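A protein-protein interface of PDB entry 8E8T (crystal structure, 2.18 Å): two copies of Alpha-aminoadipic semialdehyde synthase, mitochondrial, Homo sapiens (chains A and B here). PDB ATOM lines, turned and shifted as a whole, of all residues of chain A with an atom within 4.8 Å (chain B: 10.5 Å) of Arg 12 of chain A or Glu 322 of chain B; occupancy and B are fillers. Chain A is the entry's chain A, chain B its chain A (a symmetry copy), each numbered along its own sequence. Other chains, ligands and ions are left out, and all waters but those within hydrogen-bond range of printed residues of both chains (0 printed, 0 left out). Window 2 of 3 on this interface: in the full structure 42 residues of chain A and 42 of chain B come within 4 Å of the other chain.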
ATOM      1  N   VAL A  10       3.970  25.773  26.376  1.00  0.00           N
ATOM      2  CA  VAL A  10       4.343  24.378  26.165  1.00  0.00           C
ATOM      3  C   VAL A  10       4.438  24.164  24.661  1.00  0.00           C
ATOM      4  O   VAL A  10       3.415  24.121  23.965  1.00  0.00           O
ATOM      5  CB  VAL A  10       3.337  23.412  26.802  1.00  0.00           C
ATOM      6  CG1 VAL A  10       3.723  21.969  26.506  1.00  0.00           C
ATOM      7  CG2 VAL A  10       3.253  23.644  28.304  1.00  0.00           C
ATOM      8  N   ARG A  11       5.659  24.034  24.152  1.00  0.00           N
ATOM      9  CA  ARG A  11       5.860  23.894  22.718  1.00  0.00           C
ATOM     10  C   ARG A  11       5.440  22.506  22.238  1.00  0.00           C
ATOM     11  O   ARG A  11       5.306  21.559  23.016  1.00  0.00           O
ATOM     12  CB  ARG A  11       7.322  24.167  22.338  1.00  0.00           C
ATOM     13  CG  ARG A  11       8.299  23.059  22.709  1.00  0.00           C
ATOM     14  CD  ARG A  11       9.722  23.415  22.277  1.00  0.00           C
ATOM     15  NE  ARG A  11       9.793  23.677  20.843  1.00  0.00           N
ATOM     16  CZ  ARG A  11      10.089  22.758  19.929  1.00  0.00           C
ATOM     17  NH1 ARG A  11      10.359  21.513  20.301  1.00  0.00           N
ATOM     18  NH2 ARG A  11      10.119  23.086  18.644  1.00  0.00           N
ATOM     19  N   ARG A  12       5.227  22.408  20.929  1.00  0.00           N
ATOM     20  CA  ARG A  12       4.881  21.146  20.295  1.00  0.00           C
ATOM     21  C   ARG A  12       6.140  20.337  20.009  1.00  0.00           C
ATOM     22  O   ARG A  12       7.143  20.867  19.524  1.00  0.00           O
ATOM     23  CB  ARG A  12       4.106  21.404  19.000  1.00  0.00           C
ATOM     24  CG  ARG A  12       4.027  20.224  18.040  1.00  0.00           C
ATOM     25  CD  ARG A  12       3.293  20.604  16.763  1.00  0.00           C
ATOM     26  NE  ARG A  12       3.947  21.688  16.030  1.00  0.00           N
ATOM     27  CZ  ARG A  12       3.523  22.949  16.007  1.00  0.00           C
ATOM     28  NH1 ARG A  12       4.188  23.861  15.312  1.00  0.00           N
ATOM     29  NH2 ARG A  12       2.436  23.299  16.680  1.00  0.00           N
ATOM     30  N   GLU A  13       6.083  19.046  20.325  1.00  0.00           N
ATOM     31  CA  GLU A  13       7.204  18.147  20.091  1.00  0.00           C
ATOM     32  C   GLU A  13       7.275  17.773  18.618  1.00  0.00           C
ATOM     33  O   GLU A  13       6.266  17.402  18.012  1.00  0.00           O
ATOM     34  CB  GLU A  13       7.067  16.887  20.944  1.00  0.00           C
ATOM     35  CG  GLU A  13       6.983  17.167  22.426  1.00  0.00           C
ATOM     36  CD  GLU A  13       8.234  17.838  22.959  1.00  0.00           C
ATOM     37  OE1 GLU A  13       9.344  17.465  22.517  1.00  0.00           O
ATOM     38  OE2 GLU A  13       8.109  18.742  23.814  1.00  0.00           O
ATOM     39  N   ASP A  14       8.473  17.868  18.048  1.00  0.00           N
ATOM     40  CA  ASP A  14       8.718  17.507  16.658  1.00  0.00           C
ATOM     41  C   ASP A  14      10.012  16.712  16.525  1.00  0.00           C
ATOM     42  O   ASP A  14      10.606  16.678  15.438  1.00  0.00           O
ATOM     43  CB  ASP A  14       8.741  18.764  15.783  1.00  0.00           C
ATOM     44  CG  ASP A  14       9.758  19.771  16.255  1.00  0.00           C
ATOM     45  OD1 ASP A  14      10.348  19.552  17.336  1.00  0.00           O
ATOM     46  OD2 ASP A  14       9.968  20.781  15.553  1.00  0.00           O
ATOM     47  N   GLN A  42       0.819  25.197  22.454  1.00  0.00           N
ATOM     48  CA  GLN A  42       0.998  25.067  21.014  1.00  0.00           C
ATOM     49  C   GLN A  42       0.274  23.818  20.516  1.00  0.00           C
ATOM     50  O   GLN A  42       0.504  22.728  21.046  1.00  0.00           O
ATOM     51  CB  GLN A  42       2.480  24.997  20.672  1.00  0.00           C
ATOM     52  CG  GLN A  42       2.868  25.865  19.498  1.00  0.00           C
ATOM     53  CD  GLN A  42       4.345  25.808  19.192  1.00  0.00           C
ATOM     54  OE1 GLN A  42       5.059  24.923  19.663  1.00  0.00           O
ATOM     55  NE2 GLN A  42       4.814  26.754  18.392  1.00  0.00           N
ATOM     56  N   PRO A  43      -0.610  23.934  19.521  1.00  0.00           N
ATOM     57  CA  PRO A  43      -1.411  22.769  19.116  1.00  0.00           C
ATOM     58  C   PRO A  43      -0.541  21.640  18.583  1.00  0.00           C
ATOM     59  O   PRO A  43       0.455  21.870  17.897  1.00  0.00           O
ATOM     60  CB  PRO A  43      -2.341  23.332  18.031  1.00  0.00           C
ATOM     61  CG  PRO A  43      -1.696  24.591  17.569  1.00  0.00           C
ATOM     62  CD  PRO A  43      -0.942  25.139  18.742  1.00  0.00           C
ATOM     63  N   SER A  44      -0.928  20.410  18.917  1.00  0.00           N
ATOM     64  CA  SER A  44      -0.148  19.231  18.554  1.00  0.00           C
ATOM     65  C   SER A  44      -1.074  18.028  18.460  1.00  0.00           C
ATOM     66  O   SER A  44      -1.644  17.606  19.473  1.00  0.00           O
ATOM     67  CB  SER A  44       0.959  18.979  19.579  1.00  0.00           C
ATOM     68  OG  SER A  44       1.726  17.834  19.250  1.00  0.00           O
ATOM     69  N   GLU A  63      -0.649  28.989  18.159  1.00  0.00           N
ATOM     70  CA  GLU A  63       0.556  28.546  17.466  1.00  0.00           C
ATOM     71  C   GLU A  63       1.735  29.465  17.767  1.00  0.00           C
ATOM     72  O   GLU A  63       2.860  28.994  17.962  1.00  0.00           O
ATOM     73  CB  GLU A  63       0.291  28.461  15.963  1.00  0.00           C
ATOM     74  CG  GLU A  63       1.519  28.151  15.114  1.00  0.00           C
ATOM     75  CD  GLU A  63       2.096  26.764  15.356  1.00  0.00           C
ATOM     76  OE1 GLU A  63       1.395  25.904  15.932  1.00  0.00           O
ATOM     77  OE2 GLU A  63       3.257  26.533  14.961  1.00  0.00           O
ATOM     78  N   LYS A  81      14.101  26.848  15.236  1.00  0.00           N
ATOM     79  CA  LYS A  81      12.892  27.244  15.953  1.00  0.00           C
ATOM     80  C   LYS A  81      13.176  27.925  17.286  1.00  0.00           C
ATOM     81  O   LYS A  81      12.229  28.363  17.949  1.00  0.00           O
ATOM     82  CB  LYS A  81      11.995  26.025  16.191  1.00  0.00           C
ATOM     83  CG  LYS A  81      11.175  25.607  14.987  1.00  0.00           C
ATOM     84  CD  LYS A  81      10.004  24.736  15.404  1.00  0.00           C
ATOM     85  CE  LYS A  81       9.112  24.420  14.223  1.00  0.00           C
ATOM     86  NZ  LYS A  81       7.892  23.690  14.654  1.00  0.00           N
ATOM     87  N   LEU B 155       1.912   9.663  10.250  1.00  0.00           N
ATOM     88  CA  LEU B 155       1.508  10.913   9.625  1.00  0.00           C
ATOM     89  C   LEU B 155       1.493  12.084  10.597  1.00  0.00           C
ATOM     90  O   LEU B 155       1.277  13.221  10.165  1.00  0.00           O
ATOM     91  CB  LEU B 155       0.130  10.742   8.985  1.00  0.00           C
ATOM     92  CG  LEU B 155       0.172   9.833   7.753  1.00  0.00           C
ATOM     93  CD1 LEU B 155      -1.210   9.555   7.169  1.00  0.00           C
ATOM     94  CD2 LEU B 155       1.083  10.474   6.713  1.00  0.00           C
ATOM     95  N   GLY B 156       1.718  11.839  11.886  1.00  0.00           N
ATOM     96  CA  GLY B 156       1.757  12.886  12.884  1.00  0.00           C
ATOM     97  C   GLY B 156       0.565  12.962  13.821  1.00  0.00           C
ATOM     98  O   GLY B 156       0.467  13.930  14.583  1.00  0.00           O
ATOM     99  N   HIS B 157      -0.329  11.975  13.816  1.00  0.00           N
ATOM    100  CA  HIS B 157      -1.581  12.068  14.559  1.00  0.00           C
ATOM    101  C   HIS B 157      -1.697  10.918  15.547  1.00  0.00           C
ATOM    102  O   HIS B 157      -1.821   9.757  15.141  1.00  0.00           O
ATOM    103  CB  HIS B 157      -2.780  12.061  13.611  1.00  0.00           C
ATOM    104  CG  HIS B 157      -2.569  12.884  12.383  1.00  0.00           C
ATOM    105  ND1 HIS B 157      -2.714  14.255  12.373  1.00  0.00           N
ATOM    106  CD2 HIS B 157      -2.206  12.531  11.128  1.00  0.00           C
ATOM    107  CE1 HIS B 157      -2.451  14.711  11.162  1.00  0.00           C
ATOM    108  NE2 HIS B 157      -2.140  13.687  10.388  1.00  0.00           N
ATOM    109  N   SER B 195      -8.095  17.756  12.730  1.00  0.00           N
ATOM    110  CA  SER B 195      -7.645  18.155  11.398  1.00  0.00           C
ATOM    111  C   SER B 195      -7.715  17.015  10.381  1.00  0.00           C
ATOM    112  O   SER B 195      -7.737  17.277   9.175  1.00  0.00           O
ATOM    113  CB  SER B 195      -6.225  18.730  11.464  1.00  0.00           C
ATOM    114  OG  SER B 195      -5.259  17.749  11.800  1.00  0.00           O
ATOM    115  N   GLY B 320      -3.385  22.007   6.922  1.00  0.00           N
ATOM    116  CA  GLY B 320      -3.623  23.239   7.660  1.00  0.00           C
ATOM    117  C   GLY B 320      -2.430  23.715   8.474  1.00  0.00           C
ATOM    118  O   GLY B 320      -1.390  24.069   7.922  1.00  0.00           O
ATOM    119  N   VAL B 321      -2.588  23.724   9.801  1.00  0.00           N
ATOM    120  CA  VAL B 321      -1.503  24.166  10.674  1.00  0.00           C
ATOM    121  C   VAL B 321      -0.365  23.146  10.657  1.00  0.00           C
ATOM    122  O   VAL B 321      -0.548  21.962  10.340  1.00  0.00           O
ATOM    123  CB  VAL B 321      -2.015  24.396  12.107  1.00  0.00           C
ATOM    124  CG1 VAL B 321      -1.066  25.304  12.886  1.00  0.00           C
ATOM    125  CG2 VAL B 321      -3.428  24.967  12.089  1.00  0.00           C
ATOM    126  N   GLU B 322       0.837  23.621  11.004  1.00  0.00           N
ATOM    127  CA  GLU B 322       1.986  22.723  11.081  1.00  0.00           C
ATOM    128  C   GLU B 322       1.777  21.650  12.140  1.00  0.00           C
ATOM    129  O   GLU B 322       2.156  20.489  11.942  1.00  0.00           O
ATOM    130  CB  GLU B 322       3.259  23.511  11.385  1.00  0.00           C
ATOM    131  CG  GLU B 322       4.472  22.614  11.598  1.00  0.00           C
ATOM    132  CD  GLU B 322       5.669  23.345  12.171  1.00  0.00           C
ATOM    133  OE1 GLU B 322       5.762  24.579  11.998  1.00  0.00           O
ATOM    134  OE2 GLU B 322       6.518  22.678  12.799  1.00  0.00           O
ATOM    135  N   GLY B 323       1.179  22.020  13.274  1.00  0.00           N
ATOM    136  CA  GLY B 323       0.945  21.050  14.328  1.00  0.00           C
ATOM    137  C   GLY B 323      -0.188  20.090  14.025  1.00  0.00           C
ATOM    138  O   GLY B 323      -0.184  18.952  14.501  1.00  0.00           O
ATOM    139  N   CYS B 324      -1.169  20.524  13.238  1.00  0.00           N
ATOM    140  CA  CYS B 324      -2.371  19.736  12.967  1.00  0.00           C
ATOM    141  C   CYS B 324      -2.636  19.707  11.470  1.00  0.00           C
ATOM    142  O   CYS B 324      -3.592  20.319  10.981  1.00  0.00           O
ATOM    143  CB  CYS B 324      -3.561  20.305  13.737  1.00  0.00           C
ATOM    144  SG  CYS B 324      -3.120  20.858  15.402  1.00  0.00           S
ATOM    145  N   PRO B 325      -1.808  18.999  10.711  1.00  0.00           N
ATOM    146  CA  PRO B 325      -2.030  18.901   9.267  1.00  0.00           C
ATOM    147  C   PRO B 325      -3.238  18.038   8.939  1.00  0.00           C
ATOM    148  O   PRO B 325      -3.734  17.264   9.759  1.00  0.00           O
ATOM    149  CB  PRO B 325      -0.741  18.245   8.759  1.00  0.00           C
ATOM    150  CG  PRO B 325      -0.295  17.409   9.909  1.00  0.00           C
ATOM    151  CD  PRO B 325      -0.632  18.217  11.138  1.00  0.00           C
ATOM    152  N   ALA B 326      -3.705  18.192   7.706  1.00  0.00           N
ATOM    153  CA  ALA B 326      -4.743  17.341   7.153  1.00  0.00           C
ATOM    154  C   ALA B 326      -4.111  16.097   6.536  1.00  0.00           C
ATOM    155  O   ALA B 326      -2.898  16.033   6.321  1.00  0.00           O
ATOM    156  CB  ALA B 326      -5.557  18.101   6.104  1.00  0.00           C
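Of chain B, only Glu 322 and Gly 323 come within 4 Å of Arg 12 of chain A. Of chain A, only Arg 12 (3.5 Å) and Lys 81 (2.5 Å) come within 4 Å of Glu 322 of chain B. Arg 11 of chain A touches none of the printed residues of chain B. No residue of chain B comes within 4 Å of Glu 13 of chain A. Gln 42 of chain A touches none of the printed residues of chain B. No residue of chain B comes within 4 Å of Ser 44 of chain A. Of the printed residues of chain A, Gly 323 of chain B touches Arg 12 (3.4 Å) and Pro 43 (3.7 Å). Printed residues of chain A within 4 Å of Val 321 of chain B: Glu 63 (3.96 Å). Printed residues of chain B within 4 Å of Lys 81 of chain A: Glu 322 (2.5 Å). Pro 325 of chain B touches none of the printed residues of chain A. The nearest residue of chain B that does not touch Arg 12 of chain A is Val 321 of chain B (5.5 Å). The nearest residue of chain A that does not touch Glu 322 of chain B is Glu 63 of chain A (4.3 Å). The nearest printed residue of chain A that does not touch Cys 324 of chain B is Ser 44 of chain A (4.2 Å).
OE2 of Glu 322 of chain B lies within salt-bridge range of NZ of Lys 81 of chain A (2.5 Å). The guanidinium group of Arg 12 of chain A lies within salt-bridge range of the side-chain carboxylate of Glu 322 of chain B (3.6 Å).
The guanidinium group of Arg 12 of chain A lies within hydrogen-bond range of the backbone carbonyl oxygen of Pro 43 of chain A (2.7 Å). NE2 of Gln 42 of chain A is in hydrogen-bond range of O of Glu 63 of chain A (3.0 Å). The side-chain hydroxyl of Ser 195 of chain B lies close to the backbone carbonyl oxygen of Cys 324 of chain B (3.2 Å). The side-chain amino group (NZ) of Lys 81 of chain A lies within salt-bridge range of the side-chain carboxylate (OD2) of Asp 14 of chain A, at 3.7 Å. The backbone NH (N) of Arg 12 of chain A is in hydrogen-bond range of the side-chain amide oxygen (OE1) of Gln 42 of chain A, 2.8 Å away. The guanidinium group (NH1) of Arg 12 of chain A is in salt-bridge range of the side-chain carboxylate (OE2) of Glu 63 of chain A (2.9 Å).
Among the printed residues, pairs that only touch across the chains: Arg 12 of chain A with Gly 323 of chain B, Pro 43 of chain A with Cys 324 of chain B, Pro 43 of chain A with Gly 323 of chain B and Glu 63 of chain A with Val 321 of chain B.
Hydrophobic or aromatic side chains of chain B that line the printed part of chain A: Val 321. Along chain B the printed residues that touch a printed residue of chain A span positions 321 to 324. Of the 10 printed residues of chain A, 4 touch a printed residue of chain B. Printed residues of chain A that touch a printed residue of chain B: Arg 12, Pro 43, Glu 63 and Lys 81. Hydrophobic or aromatic side chains of chain A within 4 Å of the printed part of chain B: Pro 43. Among the printed residues, Asp or Glu carboxylates within 4 Å of a Lys or Arg side-chain nitrogen of the other chain: Arg 12 of chain A with Glu 322 of chain B and Lys 81 of chain A with Glu 322 of chain B.
No position is printed for both chains. Of the 6 pairs that touch across the chains among the printed residues, none has its exchanged pair printed and touching as well.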
